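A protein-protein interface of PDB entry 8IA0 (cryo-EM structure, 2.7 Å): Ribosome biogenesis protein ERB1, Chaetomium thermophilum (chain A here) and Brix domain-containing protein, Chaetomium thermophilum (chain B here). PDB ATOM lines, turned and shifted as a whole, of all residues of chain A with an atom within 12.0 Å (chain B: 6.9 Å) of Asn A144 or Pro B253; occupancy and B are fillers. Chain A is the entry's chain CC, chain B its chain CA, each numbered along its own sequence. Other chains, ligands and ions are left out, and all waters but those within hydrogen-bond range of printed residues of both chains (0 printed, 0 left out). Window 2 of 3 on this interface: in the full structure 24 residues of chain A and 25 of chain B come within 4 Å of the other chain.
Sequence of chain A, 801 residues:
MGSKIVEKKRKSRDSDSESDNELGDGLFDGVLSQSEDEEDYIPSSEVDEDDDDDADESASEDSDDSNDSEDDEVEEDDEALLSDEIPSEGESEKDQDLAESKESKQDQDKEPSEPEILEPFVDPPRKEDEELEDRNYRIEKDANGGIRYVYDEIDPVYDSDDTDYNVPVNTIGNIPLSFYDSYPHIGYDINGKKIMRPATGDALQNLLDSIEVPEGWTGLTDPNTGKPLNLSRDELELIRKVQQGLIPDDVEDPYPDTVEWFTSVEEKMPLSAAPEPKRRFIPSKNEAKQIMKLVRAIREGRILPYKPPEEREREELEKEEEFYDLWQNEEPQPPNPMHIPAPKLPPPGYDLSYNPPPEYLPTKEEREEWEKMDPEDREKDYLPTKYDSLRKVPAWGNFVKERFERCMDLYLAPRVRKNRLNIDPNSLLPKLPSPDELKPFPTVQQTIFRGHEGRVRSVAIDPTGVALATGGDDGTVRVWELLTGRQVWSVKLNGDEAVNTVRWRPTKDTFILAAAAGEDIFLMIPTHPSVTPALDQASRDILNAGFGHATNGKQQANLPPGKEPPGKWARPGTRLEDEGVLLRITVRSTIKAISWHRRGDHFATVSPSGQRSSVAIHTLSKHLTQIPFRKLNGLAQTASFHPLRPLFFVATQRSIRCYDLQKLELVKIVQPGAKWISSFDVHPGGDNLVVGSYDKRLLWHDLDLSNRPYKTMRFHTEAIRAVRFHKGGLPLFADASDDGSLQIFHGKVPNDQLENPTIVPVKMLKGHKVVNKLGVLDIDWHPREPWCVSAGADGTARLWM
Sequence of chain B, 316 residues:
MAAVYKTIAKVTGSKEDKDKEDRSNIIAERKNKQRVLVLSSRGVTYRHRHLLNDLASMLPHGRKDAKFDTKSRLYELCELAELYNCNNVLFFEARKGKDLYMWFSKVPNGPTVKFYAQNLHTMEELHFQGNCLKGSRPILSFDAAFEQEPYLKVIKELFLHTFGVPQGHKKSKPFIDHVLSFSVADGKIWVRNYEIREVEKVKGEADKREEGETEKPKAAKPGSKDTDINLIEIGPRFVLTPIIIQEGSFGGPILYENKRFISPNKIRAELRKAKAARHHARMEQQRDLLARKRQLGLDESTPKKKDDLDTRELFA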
ATOM      1  N   GLU A 140       2.071   4.009 -13.762  1.00  0.00           N
ATOM      2  CA  GLU A 140       2.346   5.142 -14.634  1.00  0.00           C
ATOM      3  C   GLU A 140       1.038   5.531 -15.310  1.00  0.00           C
ATOM      4  O   GLU A 140      -0.045   5.093 -14.909  1.00  0.00           O
ATOM      5  CB  GLU A 140       3.448   4.809 -15.647  1.00  0.00           C
ATOM      6  CG  GLU A 140       4.841   5.210 -15.196  1.00  0.00           C
ATOM      7  CD  GLU A 140       5.930   4.416 -15.888  1.00  0.00           C
ATOM      8  OE1 GLU A 140       5.682   3.907 -17.001  1.00  0.00           O
ATOM      9  OE2 GLU A 140       7.037   4.303 -15.321  1.00  0.00           O
ATOM     10  N   LYS A 141       1.131   6.359 -16.342  1.00  0.00           N
ATOM     11  CA  LYS A 141      -0.039   6.802 -17.082  1.00  0.00           C
ATOM     12  C   LYS A 141      -0.052   6.195 -18.478  1.00  0.00           C
ATOM     13  O   LYS A 141       0.989   6.031 -19.118  1.00  0.00           O
ATOM     14  CB  LYS A 141      -0.093   8.328 -17.179  1.00  0.00           C
ATOM     15  CG  LYS A 141      -0.113   9.033 -15.836  1.00  0.00           C
ATOM     16  CD  LYS A 141      -1.532   9.399 -15.438  1.00  0.00           C
ATOM     17  CE  LYS A 141      -2.078  10.515 -16.309  1.00  0.00           C
ATOM     18  NZ  LYS A 141      -1.030  11.514 -16.649  1.00  0.00           N
ATOM     19  N   ASP A 142      -1.253   5.859 -18.934  1.00  0.00           N
ATOM     20  CA  ASP A 142      -1.467   5.286 -20.250  1.00  0.00           C
ATOM     21  C   ASP A 142      -1.469   6.396 -21.302  1.00  0.00           C
ATOM     22  O   ASP A 142      -1.282   7.577 -20.997  1.00  0.00           O
ATOM     23  CB  ASP A 142      -2.773   4.498 -20.254  1.00  0.00           C
ATOM     24  CG  ASP A 142      -2.552   3.009 -20.383  1.00  0.00           C
ATOM     25  OD1 ASP A 142      -1.389   2.590 -20.554  1.00  0.00           O
ATOM     26  OD2 ASP A 142      -3.539   2.253 -20.268  1.00  0.00           O
ATOM     27  N   ALA A 143      -1.681   6.018 -22.563  1.00  0.00           N
ATOM     28  CA  ALA A 143      -1.754   7.006 -23.631  1.00  0.00           C
ATOM     29  C   ALA A 143      -3.105   7.699 -23.702  1.00  0.00           C
ATOM     30  O   ALA A 143      -3.213   8.749 -24.343  1.00  0.00           O
ATOM     31  CB  ALA A 143      -1.447   6.355 -24.981  1.00  0.00           C
ATOM     32  N   ASN A 144      -4.130   7.137 -23.067  1.00  0.00           N
ATOM     33  CA  ASN A 144      -5.460   7.726 -23.030  1.00  0.00           C
ATOM     34  C   ASN A 144      -5.761   8.390 -21.695  1.00  0.00           C
ATOM     35  O   ASN A 144      -6.921   8.712 -21.421  1.00  0.00           O
ATOM     36  CB  ASN A 144      -6.514   6.662 -23.337  1.00  0.00           C
ATOM     37  CG  ASN A 144      -6.471   6.202 -24.778  1.00  0.00           C
ATOM     38  OD1 ASN A 144      -5.727   6.747 -25.593  1.00  0.00           O
ATOM     39  ND2 ASN A 144      -7.269   5.193 -25.102  1.00  0.00           N
ATOM     40  N   GLY A 145      -4.747   8.600 -20.861  1.00  0.00           N
ATOM     41  CA  GLY A 145      -4.958   9.183 -19.554  1.00  0.00           C
ATOM     42  C   GLY A 145      -5.338   8.202 -18.472  1.00  0.00           C
ATOM     43  O   GLY A 145      -5.633   8.620 -17.349  1.00  0.00           O
ATOM     44  N   GLY A 146      -5.338   6.907 -18.771  1.00  0.00           N
ATOM     45  CA  GLY A 146      -5.665   5.883 -17.809  1.00  0.00           C
ATOM     46  C   GLY A 146      -4.475   5.492 -16.960  1.00  0.00           C
ATOM     47  O   GLY A 146      -3.466   6.202 -16.884  1.00  0.00           O
ATOM     48  N   ILE A 147      -4.594   4.341 -16.308  1.00  0.00           N
ATOM     49  CA  ILE A 147      -3.553   3.816 -15.435  1.00  0.00           C
ATOM     50  C   ILE A 147      -2.798   2.728 -16.182  1.00  0.00           C
ATOM     51  O   ILE A 147      -3.408   1.798 -16.726  1.00  0.00           O
ATOM     52  CB  ILE A 147      -4.146   3.273 -14.125  1.00  0.00           C
ATOM     53  CG1 ILE A 147      -4.978   4.349 -13.428  1.00  0.00           C
ATOM     54  CG2 ILE A 147      -3.041   2.793 -13.202  1.00  0.00           C
ATOM     55  CD1 ILE A 147      -5.782   3.832 -12.259  1.00  0.00           C
ATOM     56  N   ARG A 148      -1.473   2.841 -16.212  1.00  0.00           N
ATOM     57  CA  ARG A 148      -0.606   1.869 -16.863  1.00  0.00           C
ATOM     58  C   ARG A 148       0.209   1.139 -15.809  1.00  0.00           C
ATOM     59  O   ARG A 148       0.741   1.763 -14.886  1.00  0.00           O
ATOM     60  CB  ARG A 148       0.324   2.539 -17.874  1.00  0.00           C
ATOM     61  CG  ARG A 148       1.244   1.571 -18.588  1.00  0.00           C
ATOM     62  CD  ARG A 148       1.979   2.240 -19.726  1.00  0.00           C
ATOM     63  NE  ARG A 148       3.200   1.524 -20.069  1.00  0.00           N
ATOM     64  CZ  ARG A 148       3.259   0.512 -20.922  1.00  0.00           C
ATOM     65  NH1 ARG A 148       2.177   0.064 -21.539  1.00  0.00           N
ATOM     66  NH2 ARG A 148       4.430  -0.070 -21.159  1.00  0.00           N
ATOM     67  N   TYR A 149       0.310  -0.177 -15.955  1.00  0.00           N
ATOM     68  CA  TYR A 149       0.995  -1.032 -14.995  1.00  0.00           C
ATOM     69  C   TYR A 149       2.257  -1.578 -15.657  1.00  0.00           C
ATOM     70  O   TYR A 149       2.176  -2.360 -16.611  1.00  0.00           O
ATOM     71  CB  TYR A 149       0.070  -2.157 -14.534  1.00  0.00           C
ATOM     72  CG  TYR A 149      -1.162  -1.676 -13.795  1.00  0.00           C
ATOM     73  CD1 TYR A 149      -2.238  -1.127 -14.477  1.00  0.00           C
ATOM     74  CD2 TYR A 149      -1.253  -1.777 -12.420  1.00  0.00           C
ATOM     75  CE1 TYR A 149      -3.363  -0.689 -13.806  1.00  0.00           C
ATOM     76  CE2 TYR A 149      -2.373  -1.343 -11.743  1.00  0.00           C
ATOM     77  CZ  TYR A 149      -3.425  -0.801 -12.440  1.00  0.00           C
ATOM     78  OH  TYR A 149      -4.544  -0.365 -11.768  1.00  0.00           O
ATOM     79  N   VAL A 150       3.417  -1.172 -15.151  1.00  0.00           N
ATOM     80  CA  VAL A 150       4.704  -1.530 -15.737  1.00  0.00           C
ATOM     81  C   VAL A 150       5.338  -2.616 -14.881  1.00  0.00           C
ATOM     82  O   VAL A 150       5.544  -2.431 -13.676  1.00  0.00           O
ATOM     83  CB  VAL A 150       5.626  -0.307 -15.851  1.00  0.00           C
ATOM     84  CG1 VAL A 150       7.005  -0.727 -16.322  1.00  0.00           C
ATOM     85  CG2 VAL A 150       5.025   0.711 -16.801  1.00  0.00           C
ATOM     86  N   TYR A 151       5.654  -3.746 -15.503  1.00  0.00           N
ATOM     87  CA  TYR A 151       6.219  -4.898 -14.820  1.00  0.00           C
ATOM     88  C   TYR A 151       7.710  -5.011 -15.117  1.00  0.00           C
ATOM     89  O   TYR A 151       8.248  -4.347 -16.005  1.00  0.00           O
ATOM     90  CB  TYR A 151       5.492  -6.181 -15.236  1.00  0.00           C
ATOM     91  CG  TYR A 151       3.991  -6.125 -15.066  1.00  0.00           C
ATOM     92  CD1 TYR A 151       3.186  -5.522 -16.022  1.00  0.00           C
ATOM     93  CD2 TYR A 151       3.379  -6.680 -13.953  1.00  0.00           C
ATOM     94  CE1 TYR A 151       1.818  -5.466 -15.869  1.00  0.00           C
ATOM     95  CE2 TYR A 151       2.009  -6.632 -13.795  1.00  0.00           C
ATOM     96  CZ  TYR A 151       1.234  -6.023 -14.757  1.00  0.00           C
ATOM     97  OH  TYR A 151      -0.130  -5.972 -14.605  1.00  0.00           O
ATOM     98  N   ILE B 245      -2.992  -2.023 -33.202  1.00  0.00           N
ATOM     99  CA  ILE B 245      -1.770  -1.904 -32.417  1.00  0.00           C
ATOM    100  C   ILE B 245      -2.160  -1.420 -31.030  1.00  0.00           C
ATOM    101  O   ILE B 245      -2.842  -0.398 -30.895  1.00  0.00           O
ATOM    102  CB  ILE B 245      -0.761  -0.933 -33.059  1.00  0.00           C
ATOM    103  CG1 ILE B 245      -0.226  -1.498 -34.373  1.00  0.00           C
ATOM    104  CG2 ILE B 245       0.380  -0.642 -32.103  1.00  0.00           C
ATOM    105  CD1 ILE B 245       0.796  -0.608 -35.038  1.00  0.00           C
ATOM    106  N   GLN B 246      -1.729  -2.146 -30.004  1.00  0.00           N
ATOM    107  CA  GLN B 246      -2.077  -1.830 -28.627  1.00  0.00           C
ATOM    108  C   GLN B 246      -0.813  -1.727 -27.793  1.00  0.00           C
ATOM    109  O   GLN B 246       0.049  -2.608 -27.859  1.00  0.00           O
ATOM    110  CB  GLN B 246      -3.012  -2.892 -28.042  1.00  0.00           C
ATOM    111  CG  GLN B 246      -2.632  -4.315 -28.404  1.00  0.00           C
ATOM    112  CD  GLN B 246      -3.734  -5.308 -28.106  1.00  0.00           C
ATOM    113  OE1 GLN B 246      -3.961  -5.675 -26.955  1.00  0.00           O
ATOM    114  NE2 GLN B 246      -4.427  -5.752 -29.147  1.00  0.00           N
ATOM    115  N   GLU B 247      -0.701  -0.655 -27.015  1.00  0.00           N
ATOM    116  CA  GLU B 247       0.391  -0.538 -26.060  1.00  0.00           C
ATOM    117  C   GLU B 247       0.057  -1.393 -24.846  1.00  0.00           C
ATOM    118  O   GLU B 247      -1.074  -1.369 -24.349  1.00  0.00           O
ATOM    119  CB  GLU B 247       0.637   0.920 -25.676  1.00  0.00           C
ATOM    120  CG  GLU B 247      -0.360   1.519 -24.707  1.00  0.00           C
ATOM    121  CD  GLU B 247       0.264   2.566 -23.811  1.00  0.00           C
ATOM    122  OE1 GLU B 247      -0.244   3.703 -23.782  1.00  0.00           O
ATOM    123  OE2 GLU B 247       1.268   2.252 -23.138  1.00  0.00           O
ATOM    124  N   GLY B 248       1.026  -2.176 -24.390  1.00  0.00           N
ATOM    125  CA  GLY B 248       0.748  -3.217 -23.427  1.00  0.00           C
ATOM    126  C   GLY B 248       0.952  -4.571 -24.069  1.00  0.00           C
ATOM    127  O   GLY B 248       0.850  -4.697 -25.292  1.00  0.00           O
ATOM    128  N   GLY B 251      -2.935  -6.067 -24.215  1.00  0.00           N
ATOM    129  CA  GLY B 251      -4.044  -5.243 -23.787  1.00  0.00           C
ATOM    130  C   GLY B 251      -3.694  -3.775 -23.871  1.00  0.00           C
ATOM    131  O   GLY B 251      -2.936  -3.366 -24.754  1.00  0.00           O
ATOM    132  N   GLY B 252      -4.234  -2.972 -22.962  1.00  0.00           N
ATOM    133  CA  GLY B 252      -3.938  -1.562 -22.936  1.00  0.00           C
ATOM    134  C   GLY B 252      -4.687  -0.797 -24.006  1.00  0.00           C
ATOM    135  O   GLY B 252      -5.503  -1.353 -24.747  1.00  0.00           O
ATOM    136  N   PRO B 253      -4.424   0.503 -24.101  1.00  0.00           N
ATOM    137  CA  PRO B 253      -5.131   1.333 -25.080  1.00  0.00           C
ATOM    138  C   PRO B 253      -4.784   0.953 -26.507  1.00  0.00           C
ATOM    139  O   PRO B 253      -3.710   0.419 -26.794  1.00  0.00           O
ATOM    140  CB  PRO B 253      -4.649   2.752 -24.760  1.00  0.00           C
ATOM    141  CG  PRO B 253      -4.142   2.682 -23.374  1.00  0.00           C
ATOM    142  CD  PRO B 253      -3.575   1.308 -23.213  1.00  0.00           C
ATOM    143  N   ILE B 254      -5.714   1.240 -27.404  1.00  0.00           N
ATOM    144  CA  ILE B 254      -5.515   1.018 -28.829  1.00  0.00           C
ATOM    145  C   ILE B 254      -4.876   2.261 -29.427  1.00  0.00           C
ATOM    146  O   ILE B 254      -5.403   3.370 -29.291  1.00  0.00           O
ATOM    147  CB  ILE B 254      -6.845   0.691 -29.525  1.00  0.00           C
ATOM    148  CG1 ILE B 254      -7.367  -0.668 -29.055  1.00  0.00           C
ATOM    149  CG2 ILE B 254      -6.684   0.749 -31.032  1.00  0.00           C
ATOM    150  CD1 ILE B 254      -6.313  -1.747 -29.013  1.00  0.00           C
ATOM    151  N   LEU B 255      -3.737   2.078 -30.093  1.00  0.00           N
ATOM    152  CA  LEU B 255      -3.031   3.187 -30.713  1.00  0.00           C
ATOM    153  C   LEU B 255      -3.233   3.264 -32.218  1.00  0.00           C
ATOM    154  O   LEU B 255      -2.892   4.288 -32.820  1.00  0.00           O
ATOM    155  CB  LEU B 255      -1.531   3.097 -30.410  1.00  0.00           C
ATOM    156  CG  LEU B 255      -1.154   3.001 -28.933  1.00  0.00           C
ATOM    157  CD1 LEU B 255       0.355   2.954 -28.777  1.00  0.00           C
ATOM    158  CD2 LEU B 255      -1.742   4.159 -28.146  1.00  0.00           C
ATOM    159  N   TYR B 256      -3.773   2.218 -32.838  1.00  0.00           N
ATOM    160  CA  TYR B 256      -4.068   2.242 -34.262  1.00  0.00           C
ATOM    161  C   TYR B 256      -5.212   1.286 -34.558  1.00  0.00           C
ATOM    162  O   TYR B 256      -5.267   0.183 -34.013  1.00  0.00           O
ATOM    163  CB  TYR B 256      -2.846   1.861 -35.103  1.00  0.00           C
ATOM    164  CG  TYR B 256      -3.118   1.866 -36.587  1.00  0.00           C
ATOM    165  CD1 TYR B 256      -3.441   3.041 -37.248  1.00  0.00           C
ATOM    166  CD2 TYR B 256      -3.068   0.693 -37.326  1.00  0.00           C
ATOM    167  CE1 TYR B 256      -3.696   3.050 -38.604  1.00  0.00           C
ATOM    168  CE2 TYR B 256      -3.324   0.692 -38.681  1.00  0.00           C
ATOM    169  CZ  TYR B 256      -3.636   1.872 -39.315  1.00  0.00           C
ATOM    170  OH  TYR B 256      -3.890   1.876 -40.666  1.00  0.00           O
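Asp A142 touches Glu B247. Asp A142 touches Pro B253 (OD2 to CD, 3.1 Å). CB of Ala A143 touches CD2 of Leu B255 (3.9 Å). ND2 of Asn A144 touches CB of Pro B253 (3.6 Å). Gly B248 touches Arg A148.
Of the 12 printed residues of chain A, 4 touch a printed residue of chain B. Of the 10 printed residues of chain B, 4 touch a printed residue of chain A. Hydrophobic or aromatic side chains of chain B that line the printed part of chain A: Pro B253 and Leu B255. Among the printed residues, Asp or Glu carboxylates within 4 Å of a Lys or Arg side-chain nitrogen of the other chain: Arg A148 with Glu B247.
The backbone NH (N) of Glu B247 sits at hydrogen-bond distance from the backbone carbonyl oxygen (O) of Pro B253 (3.2 Å). The backbone carbonyl oxygen (O) of Ile B245 is in hydrogen-bond range of the backbone NH (N) of Leu B255, 2.8 Å away. N of Glu A140 is in hydrogen-bond range of O of Arg A148 (2.8 Å).
Of chain A, only Asp A142 (3.6 Å), Ala A143 (3.0 Å) and Arg A148 (2.9 Å) come within 4 Å of Glu B247. No residue of chain A comes within 4 Å of Gly B251. Gly B252 touches none of the printed residues of chain A. No residue of chain A comes within 4 Å of Ile B254. Leu B255 touches just one residue of chain A: Ala A143. Printed residues of chain B within 4 Å of Ala A143: Glu B247 and Leu B255. Printed residues of chain B within 4 Å of Arg A148: Glu B247 and Gly B248. Printed residues of chain B within 4 Å of Asp A142: Glu B247 and Pro B253. The nearest residue of chain A that does not touch Pro B253 is Ala A143 (4.2 Å).
N of Ala A143 sits at hydrogen-bond distance from OE1 of Glu B247 (3.0 Å). OE2 of Glu B247 lies within salt-bridge range of NH1 of Arg A148, at 2.9 Å.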
